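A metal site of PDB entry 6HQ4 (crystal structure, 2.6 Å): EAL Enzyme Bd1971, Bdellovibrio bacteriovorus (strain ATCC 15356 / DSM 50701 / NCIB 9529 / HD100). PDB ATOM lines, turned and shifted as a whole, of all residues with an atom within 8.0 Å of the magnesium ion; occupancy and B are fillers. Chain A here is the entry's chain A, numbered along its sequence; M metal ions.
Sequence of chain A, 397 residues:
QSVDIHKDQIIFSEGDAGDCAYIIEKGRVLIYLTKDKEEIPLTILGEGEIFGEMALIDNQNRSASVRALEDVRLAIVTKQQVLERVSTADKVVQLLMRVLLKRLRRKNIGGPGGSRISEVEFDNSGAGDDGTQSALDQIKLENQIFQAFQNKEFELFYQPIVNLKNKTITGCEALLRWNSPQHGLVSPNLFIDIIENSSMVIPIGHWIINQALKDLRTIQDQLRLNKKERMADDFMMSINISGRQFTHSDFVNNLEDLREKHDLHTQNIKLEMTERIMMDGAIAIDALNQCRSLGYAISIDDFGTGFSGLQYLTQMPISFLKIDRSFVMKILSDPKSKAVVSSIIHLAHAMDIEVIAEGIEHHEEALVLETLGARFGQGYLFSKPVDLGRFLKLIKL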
ATOM      1  N   GLU A 173     -30.182 -17.461 -23.536  1.00  0.00           N
ATOM      2  CA  GLU A 173     -29.130 -17.973 -22.649  1.00  0.00           C
ATOM      3  C   GLU A 173     -28.517 -19.254 -23.228  1.00  0.00           C
ATOM      4  O   GLU A 173     -29.236 -20.168 -23.626  1.00  0.00           O
ATOM      5  CB  GLU A 173     -29.676 -18.277 -21.252  1.00  0.00           C
ATOM      6  CG  GLU A 173     -28.595 -18.677 -20.247  1.00  0.00           C
ATOM      7  CD  GLU A 173     -29.123 -19.089 -18.885  1.00  0.00           C
ATOM      8  OE1 GLU A 173     -30.340 -18.957 -18.630  1.00  0.00           O
ATOM      9  OE2 GLU A 173     -28.303 -19.535 -18.059  1.00  0.00           O
ATOM     10  N   ALA A 174     -27.194 -19.311 -23.230  1.00  0.00           N
ATOM     11  CA  ALA A 174     -26.475 -20.522 -23.618  1.00  0.00           C
ATOM     12  C   ALA A 174     -26.454 -21.480 -22.439  1.00  0.00           C
ATOM     13  O   ALA A 174     -25.993 -21.138 -21.352  1.00  0.00           O
ATOM     14  CB  ALA A 174     -25.056 -20.181 -24.058  1.00  0.00           C
ATOM     15  N   LEU A 175     -26.964 -22.700 -22.660  1.00  0.00           N
ATOM     16  CA  LEU A 175     -27.008 -23.742 -21.641  1.00  0.00           C
ATOM     17  C   LEU A 175     -26.236 -24.992 -22.125  1.00  0.00           C
ATOM     18  O   LEU A 175     -26.428 -25.450 -23.251  1.00  0.00           O
ATOM     19  CB  LEU A 175     -28.454 -24.123 -21.337  1.00  0.00           C
ATOM     20  CG  LEU A 175     -29.311 -23.007 -20.732  1.00  0.00           C
ATOM     21  CD1 LEU A 175     -30.793 -23.273 -20.966  1.00  0.00           C
ATOM     22  CD2 LEU A 175     -29.008 -22.822 -19.251  1.00  0.00           C
ATOM     23  N   GLU A 196     -17.667 -26.597 -12.449  1.00  0.00           N
ATOM     24  CA  GLU A 196     -17.425 -25.255 -11.889  1.00  0.00           C
ATOM     25  C   GLU A 196     -16.441 -25.232 -10.708  1.00  0.00           C
ATOM     26  O   GLU A 196     -15.672 -24.297 -10.581  1.00  0.00           O
ATOM     27  CB  GLU A 196     -18.739 -24.586 -11.491  1.00  0.00           C
ATOM     28  CG  GLU A 196     -19.512 -24.008 -12.673  1.00  0.00           C
ATOM     29  CD  GLU A 196     -20.735 -23.206 -12.270  1.00  0.00           C
ATOM     30  OE1 GLU A 196     -20.912 -22.941 -11.061  1.00  0.00           O
ATOM     31  OE2 GLU A 196     -21.515 -22.839 -13.171  1.00  0.00           O
ATOM     32  N   SER A 238     -26.715 -14.371 -23.407  1.00  0.00           N
ATOM     33  CA  SER A 238     -26.314 -14.596 -22.010  1.00  0.00           C
ATOM     34  C   SER A 238     -25.419 -15.816 -21.892  1.00  0.00           C
ATOM     35  O   SER A 238     -25.818 -16.916 -22.257  1.00  0.00           O
ATOM     36  CB  SER A 238     -27.547 -14.823 -21.128  1.00  0.00           C
ATOM     37  OG  SER A 238     -28.118 -13.598 -20.729  1.00  0.00           O
ATOM     38  N   ILE A 239     -24.217 -15.621 -21.332  1.00  0.00           N
ATOM     39  CA  ILE A 239     -23.277 -16.718 -21.094  1.00  0.00           C
ATOM     40  C   ILE A 239     -22.978 -16.850 -19.597  1.00  0.00           C
ATOM     41  O   ILE A 239     -22.623 -15.872 -18.939  1.00  0.00           O
ATOM     42  CB  ILE A 239     -21.943 -16.489 -21.840  1.00  0.00           C
ATOM     43  CG1 ILE A 239     -22.209 -16.211 -23.326  1.00  0.00           C
ATOM     44  CG2 ILE A 239     -21.029 -17.704 -21.707  1.00  0.00           C
ATOM     45  CD1 ILE A 239     -21.013 -15.692 -24.074  1.00  0.00           C
ATOM     46  N   ASN A 240     -23.097 -18.070 -19.069  1.00  0.00           N
ATOM     47  CA  ASN A 240     -22.773 -18.344 -17.664  1.00  0.00           C
ATOM     48  C   ASN A 240     -21.262 -18.381 -17.450  1.00  0.00           C
ATOM     49  O   ASN A 240     -20.559 -19.158 -18.098  1.00  0.00           O
ATOM     50  CB  ASN A 240     -23.390 -19.676 -17.215  1.00  0.00           C
ATOM     51  CG  ASN A 240     -24.916 -19.648 -17.194  1.00  0.00           C
ATOM     52  OD1 ASN A 240     -25.517 -18.905 -16.416  1.00  0.00           O
ATOM     53  ND2 ASN A 240     -25.537 -20.447 -18.047  1.00  0.00           N
ATOM     54  N   ILE A 241     -20.775 -17.544 -16.539  1.00  0.00           N
ATOM     55  CA  ILE A 241     -19.350 -17.468 -16.193  1.00  0.00           C
ATOM     56  C   ILE A 241     -19.208 -17.814 -14.707  1.00  0.00           C
ATOM     57  O   ILE A 241     -19.772 -17.139 -13.861  1.00  0.00           O
ATOM     58  CB  ILE A 241     -18.796 -16.035 -16.430  1.00  0.00           C
ATOM     59  CG1 ILE A 241     -18.997 -15.610 -17.888  1.00  0.00           C
ATOM     60  CG2 ILE A 241     -17.333 -15.941 -16.016  1.00  0.00           C
ATOM     61  CD1 ILE A 241     -18.365 -16.521 -18.918  1.00  0.00           C
ATOM     62  N   GLU A 272     -23.523 -13.897 -17.154  1.00  0.00           N
ATOM     63  CA  GLU A 272     -24.279 -14.363 -15.991  1.00  0.00           C
ATOM     64  C   GLU A 272     -23.348 -14.900 -14.902  1.00  0.00           C
ATOM     65  O   GLU A 272     -22.570 -15.817 -15.156  1.00  0.00           O
ATOM     66  CB  GLU A 272     -25.300 -15.423 -16.389  1.00  0.00           C
ATOM     67  CG  GLU A 272     -26.397 -14.912 -17.307  1.00  0.00           C
ATOM     68  CD  GLU A 272     -27.544 -15.879 -17.455  1.00  0.00           C
ATOM     69  OE1 GLU A 272     -27.419 -17.046 -17.002  1.00  0.00           O
ATOM     70  OE2 GLU A 272     -28.581 -15.479 -18.015  1.00  0.00           O
ATOM     71  N   MET A 273     -23.442 -14.327 -13.700  1.00  0.00           N
ATOM     72  CA  MET A 273     -22.545 -14.660 -12.591  1.00  0.00           C
ATOM     73  C   MET A 273     -23.336 -14.988 -11.329  1.00  0.00           C
ATOM     74  O   MET A 273     -24.414 -14.445 -11.110  1.00  0.00           O
ATOM     75  CB  MET A 273     -21.637 -13.472 -12.265  1.00  0.00           C
ATOM     76  CG  MET A 273     -21.028 -12.800 -13.484  1.00  0.00           C
ATOM     77  SD  MET A 273     -19.304 -12.336 -13.239  1.00  0.00           S
ATOM     78  CE  MET A 273     -18.644 -12.551 -14.891  1.00  0.00           C
ATOM     79  N   SER A 299     -24.847  -9.616 -15.207  1.00  0.00           N
ATOM     80  CA  SER A 299     -26.118 -10.105 -14.675  1.00  0.00           C
ATOM     81  C   SER A 299     -25.862 -11.047 -13.506  1.00  0.00           C
ATOM     82  O   SER A 299     -24.969 -11.888 -13.567  1.00  0.00           O
ATOM     83  CB  SER A 299     -26.888 -10.832 -15.766  1.00  0.00           C
ATOM     84  OG  SER A 299     -28.020 -11.502 -15.244  1.00  0.00           O
ATOM     85  N   ILE A 300     -26.649 -10.912 -12.442  1.00  0.00           N
ATOM     86  CA  ILE A 300     -26.529 -11.782 -11.271  1.00  0.00           C
ATOM     87  C   ILE A 300     -27.545 -12.911 -11.381  1.00  0.00           C
ATOM     88  O   ILE A 300     -28.754 -12.678 -11.321  1.00  0.00           O
ATOM     89  CB  ILE A 300     -26.753 -11.008  -9.957  1.00  0.00           C
ATOM     90  CG1 ILE A 300     -25.678  -9.923  -9.787  1.00  0.00           C
ATOM     91  CG2 ILE A 300     -26.734 -11.949  -8.759  1.00  0.00           C
ATOM     92  CD1 ILE A 300     -24.257 -10.422  -9.716  1.00  0.00           C
ATOM     93  N   ASP A 301     -27.038 -14.113 -11.539  1.00  0.00           N
ATOM     94  CA  ASP A 301     -27.865 -15.302 -11.743  1.00  0.00           C
ATOM     95  C   ASP A 301     -28.286 -15.851 -10.382  1.00  0.00           C
ATOM     96  O   ASP A 301     -27.548 -15.748  -9.400  1.00  0.00           O
ATOM     97  CB  ASP A 301     -27.060 -16.361 -12.510  1.00  0.00           C
ATOM     98  CG  ASP A 301     -27.941 -17.264 -13.349  1.00  0.00           C
ATOM     99  OD1 ASP A 301     -29.171 -17.278 -13.152  1.00  0.00           O
ATOM    100  OD2 ASP A 301     -27.401 -17.966 -14.238  1.00  0.00           O
ATOM    101  N   ASP A 302     -29.477 -16.441 -10.336  1.00  0.00           N
ATOM    102  CA  ASP A 302     -29.980 -17.040  -9.101  1.00  0.00           C
ATOM    103  C   ASP A 302     -29.857 -16.086  -7.914  1.00  0.00           C
ATOM    104  O   ASP A 302     -29.286 -16.429  -6.868  1.00  0.00           O
ATOM    105  CB  ASP A 302     -29.255 -18.371  -8.802  1.00  0.00           C
ATOM    106  CG  ASP A 302     -29.320 -19.364  -9.950  1.00  0.00           C
ATOM    107  OD1 ASP A 302     -30.027 -19.099 -10.957  1.00  0.00           O
ATOM    108  OD2 ASP A 302     -28.664 -20.426  -9.853  1.00  0.00           O
ATOM    109  N   LYS A 322     -31.503 -12.206 -12.207  1.00  0.00           N
ATOM    110  CA  LYS A 322     -32.458 -13.228 -12.573  1.00  0.00           C
ATOM    111  C   LYS A 322     -33.089 -13.822 -11.326  1.00  0.00           C
ATOM    112  O   LYS A 322     -32.401 -14.352 -10.448  1.00  0.00           O
ATOM    113  CB  LYS A 322     -31.766 -14.325 -13.393  1.00  0.00           C
ATOM    114  CG  LYS A 322     -30.972 -13.789 -14.565  1.00  0.00           C
ATOM    115  CD  LYS A 322     -30.463 -14.905 -15.465  1.00  0.00           C
ATOM    116  CE  LYS A 322     -31.518 -15.363 -16.456  1.00  0.00           C
ATOM    117  NZ  LYS A 322     -31.034 -16.492 -17.299  1.00  0.00           N
ATOM    118  N   ASP A 324     -34.601 -16.637  -9.578  1.00  0.00           N
ATOM    119  CA  ASP A 324     -34.467 -18.095  -9.739  1.00  0.00           C
ATOM    120  C   ASP A 324     -35.824 -18.783  -9.843  1.00  0.00           C
ATOM    121  O   ASP A 324     -36.825 -18.288  -9.344  1.00  0.00           O
ATOM    122  CB  ASP A 324     -33.694 -18.642  -8.530  1.00  0.00           C
ATOM    123  CG  ASP A 324     -33.379 -20.120  -8.658  1.00  0.00           C
ATOM    124  OD1 ASP A 324     -32.891 -20.548  -9.725  1.00  0.00           O
ATOM    125  OD2 ASP A 324     -33.635 -20.861  -7.691  1.00  0.00           O
ATOM    126  N   ARG A 325     -35.846 -19.940 -10.519  1.00  0.00           N
ATOM    127  CA  ARG A 325     -37.077 -20.704 -10.710  1.00  0.00           C
ATOM    128  C   ARG A 325     -37.717 -21.191  -9.405  1.00  0.00           C
ATOM    129  O   ARG A 325     -38.939 -21.331  -9.336  1.00  0.00           O
ATOM    130  CB  ARG A 325     -36.822 -21.907 -11.637  1.00  0.00           C
ATOM    131  CG  ARG A 325     -35.911 -22.982 -11.057  1.00  0.00           C
ATOM    132  CD  ARG A 325     -35.316 -23.882 -12.139  1.00  0.00           C
ATOM    133  NE  ARG A 325     -34.547 -23.118 -13.126  1.00  0.00           N
ATOM    134  CZ  ARG A 325     -34.857 -22.977 -14.420  1.00  0.00           C
ATOM    135  NH1 ARG A 325     -35.933 -23.558 -14.948  1.00  0.00           N
ATOM    136  NH2 ARG A 325     -34.071 -22.246 -15.204  1.00  0.00           N
ATOM    137  N   GLU A 358     -37.218 -16.381 -14.340  1.00  0.00           N
ATOM    138  CA  GLU A 358     -37.069 -17.661 -15.025  1.00  0.00           C
ATOM    139  C   GLU A 358     -37.905 -18.768 -14.384  1.00  0.00           C
ATOM    140  O   GLU A 358     -38.429 -18.598 -13.284  1.00  0.00           O
ATOM    141  CB  GLU A 358     -35.589 -18.078 -15.156  1.00  0.00           C
ATOM    142  CG  GLU A 358     -34.782 -18.084 -13.878  1.00  0.00           C
ATOM    143  CD  GLU A 358     -33.367 -18.602 -14.095  1.00  0.00           C
ATOM    144  OE1 GLU A 358     -32.687 -18.097 -15.011  1.00  0.00           O
ATOM    145  OE2 GLU A 358     -32.931 -19.502 -13.345  1.00  0.00           O
ATOM    146  N   GLN A 378     -38.175 -16.037 -18.922  1.00  0.00           N
ATOM    147  CA  GLN A 378     -37.835 -17.238 -19.685  1.00  0.00           C
ATOM    148  C   GLN A 378     -38.384 -18.483 -19.026  1.00  0.00           C
ATOM    149  O   GLN A 378     -38.507 -18.547 -17.808  1.00  0.00           O
ATOM    150  CB  GLN A 378     -36.322 -17.354 -19.958  1.00  0.00           C
ATOM    151  CG  GLN A 378     -35.444 -17.677 -18.761  1.00  0.00           C
ATOM    152  CD  GLN A 378     -34.004 -17.924 -19.169  1.00  0.00           C
ATOM    153  OE1 GLN A 378     -33.154 -17.050 -19.057  1.00  0.00           O
ATOM    154  NE2 GLN A 378     -33.723 -19.137 -19.645  1.00  0.00           N
HETATM  155 MG    MG M   1     -27.982 -19.004 -15.818  1.00  0.00          MG
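N of Ile 241 is in hydrogen-bond range of O of Glu 272, at 2.8 Å. The side-chain carboxylate (OE1) of Glu 173 lies close to the side-chain amide oxygen (OE1) of Gln 378. The backbone NH (N) of Asp 301 lies within hydrogen-bond range of the backbone carbonyl oxygen (O) of Met 273 (2.7 Å). The side-chain hydroxyl (OG) of Ser 238 sits at hydrogen-bond distance from the side-chain carboxylate (OE2) of Glu 272 (3.3 Å). The side-chain amide nitrogen (ND2) of Asn 240 sits at hydrogen-bond distance from the backbone carbonyl oxygen (O) of Ala 174 (3.4 Å). N of Glu 272 sits at hydrogen-bond distance from O of Ile 239 (2.8 Å). OE2 of Glu 272 lies within salt-bridge range of NZ of Lys 322 (2.7 Å). OE1 of Glu 173 lies within salt-bridge range of NZ of Lys 322.
Of the 19 residues printed, 4 come within 4 Å of the magnesium ion.
The magnesium ion is bound by OD2 of Asp 301 (2.0 Å), OE2 of Glu 173 (2.3 Å), OE1 of Glu 272 (2.4 Å) and OD1 of Asn 240 (2.5 Å).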
